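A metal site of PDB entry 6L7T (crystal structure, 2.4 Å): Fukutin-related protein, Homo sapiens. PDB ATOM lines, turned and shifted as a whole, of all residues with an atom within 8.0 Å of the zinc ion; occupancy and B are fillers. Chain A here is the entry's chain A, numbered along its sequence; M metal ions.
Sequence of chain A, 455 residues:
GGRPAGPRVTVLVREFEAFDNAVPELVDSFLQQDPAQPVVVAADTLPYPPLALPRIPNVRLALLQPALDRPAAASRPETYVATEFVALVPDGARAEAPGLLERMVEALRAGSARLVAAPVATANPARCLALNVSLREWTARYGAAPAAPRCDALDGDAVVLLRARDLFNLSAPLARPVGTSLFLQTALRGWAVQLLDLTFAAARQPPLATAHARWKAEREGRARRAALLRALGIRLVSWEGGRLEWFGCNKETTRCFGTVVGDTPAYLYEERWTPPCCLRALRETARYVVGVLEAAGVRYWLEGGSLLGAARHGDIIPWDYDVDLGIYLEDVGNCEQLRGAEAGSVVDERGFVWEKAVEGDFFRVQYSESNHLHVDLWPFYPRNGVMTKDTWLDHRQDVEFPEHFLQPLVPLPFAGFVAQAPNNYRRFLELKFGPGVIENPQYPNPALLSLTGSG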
ATOM      1  N   ARG A 235      -9.676 -19.052  12.874  1.00  0.00           N
ATOM      2  CA  ARG A 235      -8.442 -19.387  13.575  1.00  0.00           C
ATOM      3  C   ARG A 235      -7.488 -18.211  13.681  1.00  0.00           C
ATOM      4  O   ARG A 235      -6.548 -18.259  14.488  1.00  0.00           O
ATOM      5  CB  ARG A 235      -7.711 -20.533  12.869  1.00  0.00           C
ATOM      6  CG  ARG A 235      -8.475 -21.835  12.828  1.00  0.00           C
ATOM      7  CD  ARG A 235      -8.202 -22.677  14.069  1.00  0.00           C
ATOM      8  NE  ARG A 235      -8.688 -24.040  13.878  1.00  0.00           N
ATOM      9  CZ  ARG A 235      -9.940 -24.417  14.093  1.00  0.00           C
ATOM     10  NH1 ARG A 235     -10.837 -23.544  14.514  1.00  0.00           N
ATOM     11  NH2 ARG A 235     -10.296 -25.677  13.875  1.00  0.00           N
ATOM     12  N   TRP A 246      -4.217 -15.365  17.277  1.00  0.00           N
ATOM     13  CA  TRP A 246      -4.373 -16.768  16.916  1.00  0.00           C
ATOM     14  C   TRP A 246      -5.325 -17.493  17.856  1.00  0.00           C
ATOM     15  O   TRP A 246      -5.387 -17.215  19.062  1.00  0.00           O
ATOM     16  CB  TRP A 246      -3.027 -17.506  16.925  1.00  0.00           C
ATOM     17  CG  TRP A 246      -2.037 -17.034  15.902  1.00  0.00           C
ATOM     18  CD1 TRP A 246      -0.984 -16.179  16.104  1.00  0.00           C
ATOM     19  CD2 TRP A 246      -1.982 -17.404  14.515  1.00  0.00           C
ATOM     20  NE1 TRP A 246      -0.285 -15.992  14.940  1.00  0.00           N
ATOM     21  CE2 TRP A 246      -0.879 -16.736  13.945  1.00  0.00           C
ATOM     22  CE3 TRP A 246      -2.763 -18.230  13.696  1.00  0.00           C
ATOM     23  CZ2 TRP A 246      -0.532 -16.860  12.601  1.00  0.00           C
ATOM     24  CZ3 TRP A 246      -2.412 -18.362  12.351  1.00  0.00           C
ATOM     25  CH2 TRP A 246      -1.310 -17.680  11.824  1.00  0.00           C
ATOM     26  N   PHE A 247      -6.066 -18.448  17.277  1.00  0.00           N
ATOM     27  CA  PHE A 247      -7.124 -19.172  17.968  1.00  0.00           C
ATOM     28  C   PHE A 247      -7.126 -20.640  17.547  1.00  0.00           C
ATOM     29  O   PHE A 247      -8.182 -21.279  17.543  1.00  0.00           O
ATOM     30  CB  PHE A 247      -8.488 -18.518  17.696  1.00  0.00           C
ATOM     31  CG  PHE A 247      -8.586 -17.110  18.208  1.00  0.00           C
ATOM     32  CD1 PHE A 247      -8.914 -16.881  19.536  1.00  0.00           C
ATOM     33  CD2 PHE A 247      -8.317 -16.033  17.385  1.00  0.00           C
ATOM     34  CE1 PHE A 247      -8.986 -15.578  20.035  1.00  0.00           C
ATOM     35  CE2 PHE A 247      -8.384 -14.728  17.872  1.00  0.00           C
ATOM     36  CZ  PHE A 247      -8.729 -14.505  19.206  1.00  0.00           C
ATOM     37  N   GLY A 248      -5.960 -21.183  17.200  1.00  0.00           N
ATOM     38  CA  GLY A 248      -5.844 -22.544  16.693  1.00  0.00           C
ATOM     39  C   GLY A 248      -4.886 -23.362  17.534  1.00  0.00           C
ATOM     40  O   GLY A 248      -4.901 -23.318  18.761  1.00  0.00           O
ATOM     41  N   CYS A 249      -4.042 -24.127  16.845  1.00  0.00           N
ATOM     42  CA  CYS A 249      -3.074 -25.018  17.478  1.00  0.00           C
ATOM     43  C   CYS A 249      -1.722 -24.328  17.626  1.00  0.00           C
ATOM     44  O   CYS A 249      -1.477 -23.239  17.091  1.00  0.00           O
ATOM     45  CB  CYS A 249      -2.952 -26.309  16.670  1.00  0.00           C
ATOM     46  SG  CYS A 249      -2.150 -26.145  15.050  1.00  0.00           S
ATOM     47  N   ASN A 250      -0.833 -24.975  18.378  1.00  0.00           N
ATOM     48  CA  ASN A 250       0.488 -24.402  18.655  1.00  0.00           C
ATOM     49  C   ASN A 250       1.405 -25.505  19.164  1.00  0.00           C
ATOM     50  O   ASN A 250       1.052 -26.684  19.193  1.00  0.00           O
ATOM     51  CB  ASN A 250       0.396 -23.236  19.652  1.00  0.00           C
ATOM     52  CG  ASN A 250      -0.203 -23.649  20.987  1.00  0.00           C
ATOM     53  OD1 ASN A 250       0.310 -24.535  21.664  1.00  0.00           O
ATOM     54  ND2 ASN A 250      -1.291 -22.997  21.360  1.00  0.00           N
ATOM     55  N   THR A 253      -0.123 -27.847  21.805  1.00  0.00           N
ATOM     56  CA  THR A 253      -1.387 -28.516  21.580  1.00  0.00           C
ATOM     57  C   THR A 253      -1.231 -29.572  20.507  1.00  0.00           C
ATOM     58  O   THR A 253      -0.184 -29.705  19.859  1.00  0.00           O
ATOM     59  CB  THR A 253      -2.485 -27.517  21.203  1.00  0.00           C
ATOM     60  OG1 THR A 253      -2.371 -27.129  19.828  1.00  0.00           O
ATOM     61  CG2 THR A 253      -2.401 -26.285  22.102  1.00  0.00           C
ATOM     62  N   THR A 254      -2.290 -30.358  20.330  1.00  0.00           N
ATOM     63  CA  THR A 254      -2.413 -31.210  19.164  1.00  0.00           C
ATOM     64  C   THR A 254      -2.713 -30.347  17.933  1.00  0.00           C
ATOM     65  O   THR A 254      -3.190 -29.215  18.049  1.00  0.00           O
ATOM     66  CB  THR A 254      -3.507 -32.250  19.382  1.00  0.00           C
ATOM     67  OG1 THR A 254      -3.573 -33.129  18.246  1.00  0.00           O
ATOM     68  CG2 THR A 254      -4.847 -31.568  19.541  1.00  0.00           C
ATOM     69  N   ARG A 255      -2.398 -30.882  16.755  1.00  0.00           N
ATOM     70  CA  ARG A 255      -2.748 -30.148  15.552  1.00  0.00           C
ATOM     71  C   ARG A 255      -4.262 -30.149  15.359  1.00  0.00           C
ATOM     72  O   ARG A 255      -4.985 -30.998  15.888  1.00  0.00           O
ATOM     73  CB  ARG A 255      -2.040 -30.718  14.319  1.00  0.00           C
ATOM     74  CG  ARG A 255      -2.632 -31.998  13.753  1.00  0.00           C
ATOM     75  CD  ARG A 255      -1.723 -32.584  12.668  1.00  0.00           C
ATOM     76  NE  ARG A 255      -2.115 -33.938  12.280  1.00  0.00           N
ATOM     77  CZ  ARG A 255      -1.394 -34.721  11.488  1.00  0.00           C
ATOM     78  NH1 ARG A 255      -0.248 -34.294  10.984  1.00  0.00           N
ATOM     79  NH2 ARG A 255      -1.831 -35.942  11.185  1.00  0.00           N
ATOM     80  N   CYS A 256      -4.739 -29.161  14.584  1.00  0.00           N
ATOM     81  CA  CYS A 256      -6.177 -28.924  14.484  1.00  0.00           C
ATOM     82  C   CYS A 256      -6.919 -30.156  13.965  1.00  0.00           C
ATOM     83  O   CYS A 256      -7.932 -30.568  14.537  1.00  0.00           O
ATOM     84  CB  CYS A 256      -6.437 -27.721  13.577  1.00  0.00           C
ATOM     85  SG  CYS A 256      -5.929 -26.135  14.255  1.00  0.00           S
ATOM     86  N   PHE A 257      -6.436 -30.764  12.882  1.00  0.00           N
ATOM     87  CA  PHE A 257      -7.177 -31.838  12.236  1.00  0.00           C
ATOM     88  C   PHE A 257      -6.834 -33.213  12.777  1.00  0.00           C
ATOM     89  O   PHE A 257      -7.413 -34.204  12.318  1.00  0.00           O
ATOM     90  CB  PHE A 257      -6.997 -31.800  10.712  1.00  0.00           C
ATOM     91  CG  PHE A 257      -5.567 -31.728  10.242  1.00  0.00           C
ATOM     92  CD1 PHE A 257      -4.918 -30.508  10.133  1.00  0.00           C
ATOM     93  CD2 PHE A 257      -4.885 -32.880   9.887  1.00  0.00           C
ATOM     94  CE1 PHE A 257      -3.604 -30.438   9.686  1.00  0.00           C
ATOM     95  CE2 PHE A 257      -3.574 -32.833   9.441  1.00  0.00           C
ATOM     96  CZ  PHE A 257      -2.924 -31.603   9.343  1.00  0.00           C
ATOM     97  N   THR A 274      -6.365 -25.692   4.602  1.00  0.00           N
ATOM     98  CA  THR A 274      -5.579 -25.960   5.796  1.00  0.00           C
ATOM     99  C   THR A 274      -5.697 -24.779   6.771  1.00  0.00           C
ATOM    100  O   THR A 274      -5.592 -23.629   6.355  1.00  0.00           O
ATOM    101  CB  THR A 274      -4.115 -26.195   5.448  1.00  0.00           C
ATOM    102  OG1 THR A 274      -4.011 -27.254   4.479  1.00  0.00           O
ATOM    103  CG2 THR A 274      -3.321 -26.589   6.711  1.00  0.00           C
ATOM    104  N   PRO A 275      -5.934 -25.036   8.056  1.00  0.00           N
ATOM    105  CA  PRO A 275      -5.963 -23.943   9.050  1.00  0.00           C
ATOM    106  C   PRO A 275      -4.670 -23.153   9.030  1.00  0.00           C
ATOM    107  O   PRO A 275      -3.571 -23.713   8.847  1.00  0.00           O
ATOM    108  CB  PRO A 275      -6.142 -24.690  10.379  1.00  0.00           C
ATOM    109  CG  PRO A 275      -6.892 -25.924   9.991  1.00  0.00           C
ATOM    110  CD  PRO A 275      -6.376 -26.316   8.621  1.00  0.00           C
ATOM    111  N   PRO A 276      -4.754 -21.829   9.213  1.00  0.00           N
ATOM    112  CA  PRO A 276      -3.546 -21.000   9.098  1.00  0.00           C
ATOM    113  C   PRO A 276      -2.548 -21.246  10.212  1.00  0.00           C
ATOM    114  O   PRO A 276      -1.340 -21.076   9.989  1.00  0.00           O
ATOM    115  CB  PRO A 276      -4.093 -19.571   9.139  1.00  0.00           C
ATOM    116  CG  PRO A 276      -5.425 -19.693   9.816  1.00  0.00           C
ATOM    117  CD  PRO A 276      -5.969 -21.040   9.455  1.00  0.00           C
ATOM    118  N   CYS A 277      -3.010 -21.631  11.398  1.00  0.00           N
ATOM    119  CA  CYS A 277      -2.096 -22.008  12.478  1.00  0.00           C
ATOM    120  C   CYS A 277      -1.303 -23.248  12.111  1.00  0.00           C
ATOM    121  O   CYS A 277      -0.113 -23.361  12.447  1.00  0.00           O
ATOM    122  CB  CYS A 277      -2.883 -22.266  13.759  1.00  0.00           C
ATOM    123  SG  CYS A 277      -4.353 -23.293  13.446  1.00  0.00           S
ATOM    124  N   CYS A 278      -1.948 -24.197  11.431  1.00  0.00           N
ATOM    125  CA  CYS A 278      -1.249 -25.402  10.972  1.00  0.00           C
ATOM    126  C   CYS A 278      -0.231 -25.060   9.883  1.00  0.00           C
ATOM    127  O   CYS A 278       0.874 -25.631   9.858  1.00  0.00           O
ATOM    128  CB  CYS A 278      -2.249 -26.438  10.469  1.00  0.00           C
ATOM    129  SG  CYS A 278      -3.449 -27.056  11.687  1.00  0.00           S
ATOM    130  N   LEU A 279      -0.577 -24.145   8.981  1.00  0.00           N
ATOM    131  CA  LEU A 279       0.376 -23.719   7.961  1.00  0.00           C
ATOM    132  C   LEU A 279       1.525 -22.947   8.574  1.00  0.00           C
ATOM    133  O   LEU A 279       2.686 -23.117   8.160  1.00  0.00           O
ATOM    134  CB  LEU A 279      -0.333 -22.876   6.898  1.00  0.00           C
ATOM    135  CG  LEU A 279      -1.260 -23.636   5.943  1.00  0.00           C
ATOM    136  CD1 LEU A 279      -2.002 -22.665   5.023  1.00  0.00           C
ATOM    137  CD2 LEU A 279      -0.479 -24.663   5.135  1.00  0.00           C
ATOM    138  N   ARG A 280       1.230 -22.098   9.569  1.00  0.00           N
ATOM    139  CA  ARG A 280       2.290 -21.356  10.247  1.00  0.00           C
ATOM    140  C   ARG A 280       3.293 -22.290  10.897  1.00  0.00           C
ATOM    141  O   ARG A 280       4.506 -22.101  10.770  1.00  0.00           O
ATOM    142  CB  ARG A 280       1.672 -20.426  11.291  1.00  0.00           C
ATOM    143  CG  ARG A 280       2.644 -19.403  11.891  1.00  0.00           C
ATOM    144  CD  ARG A 280       2.272 -19.100  13.333  1.00  0.00           C
ATOM    145  NE  ARG A 280       2.236 -20.325  14.129  1.00  0.00           N
ATOM    146  CZ  ARG A 280       3.309 -20.923  14.630  1.00  0.00           C
ATOM    147  NH1 ARG A 280       4.515 -20.415  14.435  1.00  0.00           N
ATOM    148  NH2 ARG A 280       3.178 -22.042  15.346  1.00  0.00           N
ATOM    149  N   ALA A 281       2.810 -23.335  11.578  1.00  0.00           N
ATOM    150  CA  ALA A 281       3.713 -24.291  12.212  1.00  0.00           C
ATOM    151  C   ALA A 281       4.501 -25.076  11.170  1.00  0.00           C
ATOM    152  O   ALA A 281       5.658 -25.422  11.408  1.00  0.00           O
ATOM    153  CB  ALA A 281       2.933 -25.249  13.114  1.00  0.00           C
ATOM    154  N   ASN A 371       2.152 -31.742  18.804  1.00  0.00           N
ATOM    155  CA  ASN A 371       1.658 -31.230  17.524  1.00  0.00           C
ATOM    156  C   ASN A 371       2.421 -31.937  16.407  1.00  0.00           C
ATOM    157  O   ASN A 371       3.624 -31.734  16.240  1.00  0.00           O
ATOM    158  CB  ASN A 371       1.844 -29.717  17.446  1.00  0.00           C
ATOM    159  CG  ASN A 371       1.113 -29.089  16.270  1.00  0.00           C
ATOM    160  OD1 ASN A 371       1.100 -29.645  15.173  1.00  0.00           O
ATOM    161  ND2 ASN A 371       0.500 -27.938  16.502  1.00  0.00           N
ATOM    162  N   LEU A 373       2.216 -31.869  13.007  1.00  0.00           N
ATOM    163  CA  LEU A 373       2.577 -31.309  11.712  1.00  0.00           C
ATOM    164  C   LEU A 373       4.047 -31.606  11.435  1.00  0.00           C
ATOM    165  O   LEU A 373       4.889 -31.477  12.325  1.00  0.00           O
ATOM    166  CB  LEU A 373       2.303 -29.809  11.703  1.00  0.00           C
ATOM    167  CG  LEU A 373       0.813 -29.499  11.849  1.00  0.00           C
ATOM    168  CD1 LEU A 373       0.578 -28.095  12.359  1.00  0.00           C
ATOM    169  CD2 LEU A 373       0.078 -29.719  10.531  1.00  0.00           C
HETATM  170 ZN    ZN M   1      -3.771 -25.556  13.474  1.00  0.00          ZN
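The zinc ion is bound by the side-chain sulfur of Cys 277 (2.3 Å), the side-chain sulfur of Cys 249 (2.3 Å), the side-chain sulfur of Cys 278 (2.4 Å) and the side-chain sulfur of Cys 256 (2.4 Å).
The zinc ion has four donor atoms within binding distance.
Pro 275 touches the zinc ion (CB to ZN, 3.99 Å).
Of the 21 residues printed, 5 come within 4 Å of the zinc ion.
SG of Cys 249 lies close to ND2 of Asn 371 (3.5 Å).
The side-chain sulfur of Cys 256 lies close to the guanidinium group of Arg 235 (3.5 Å).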
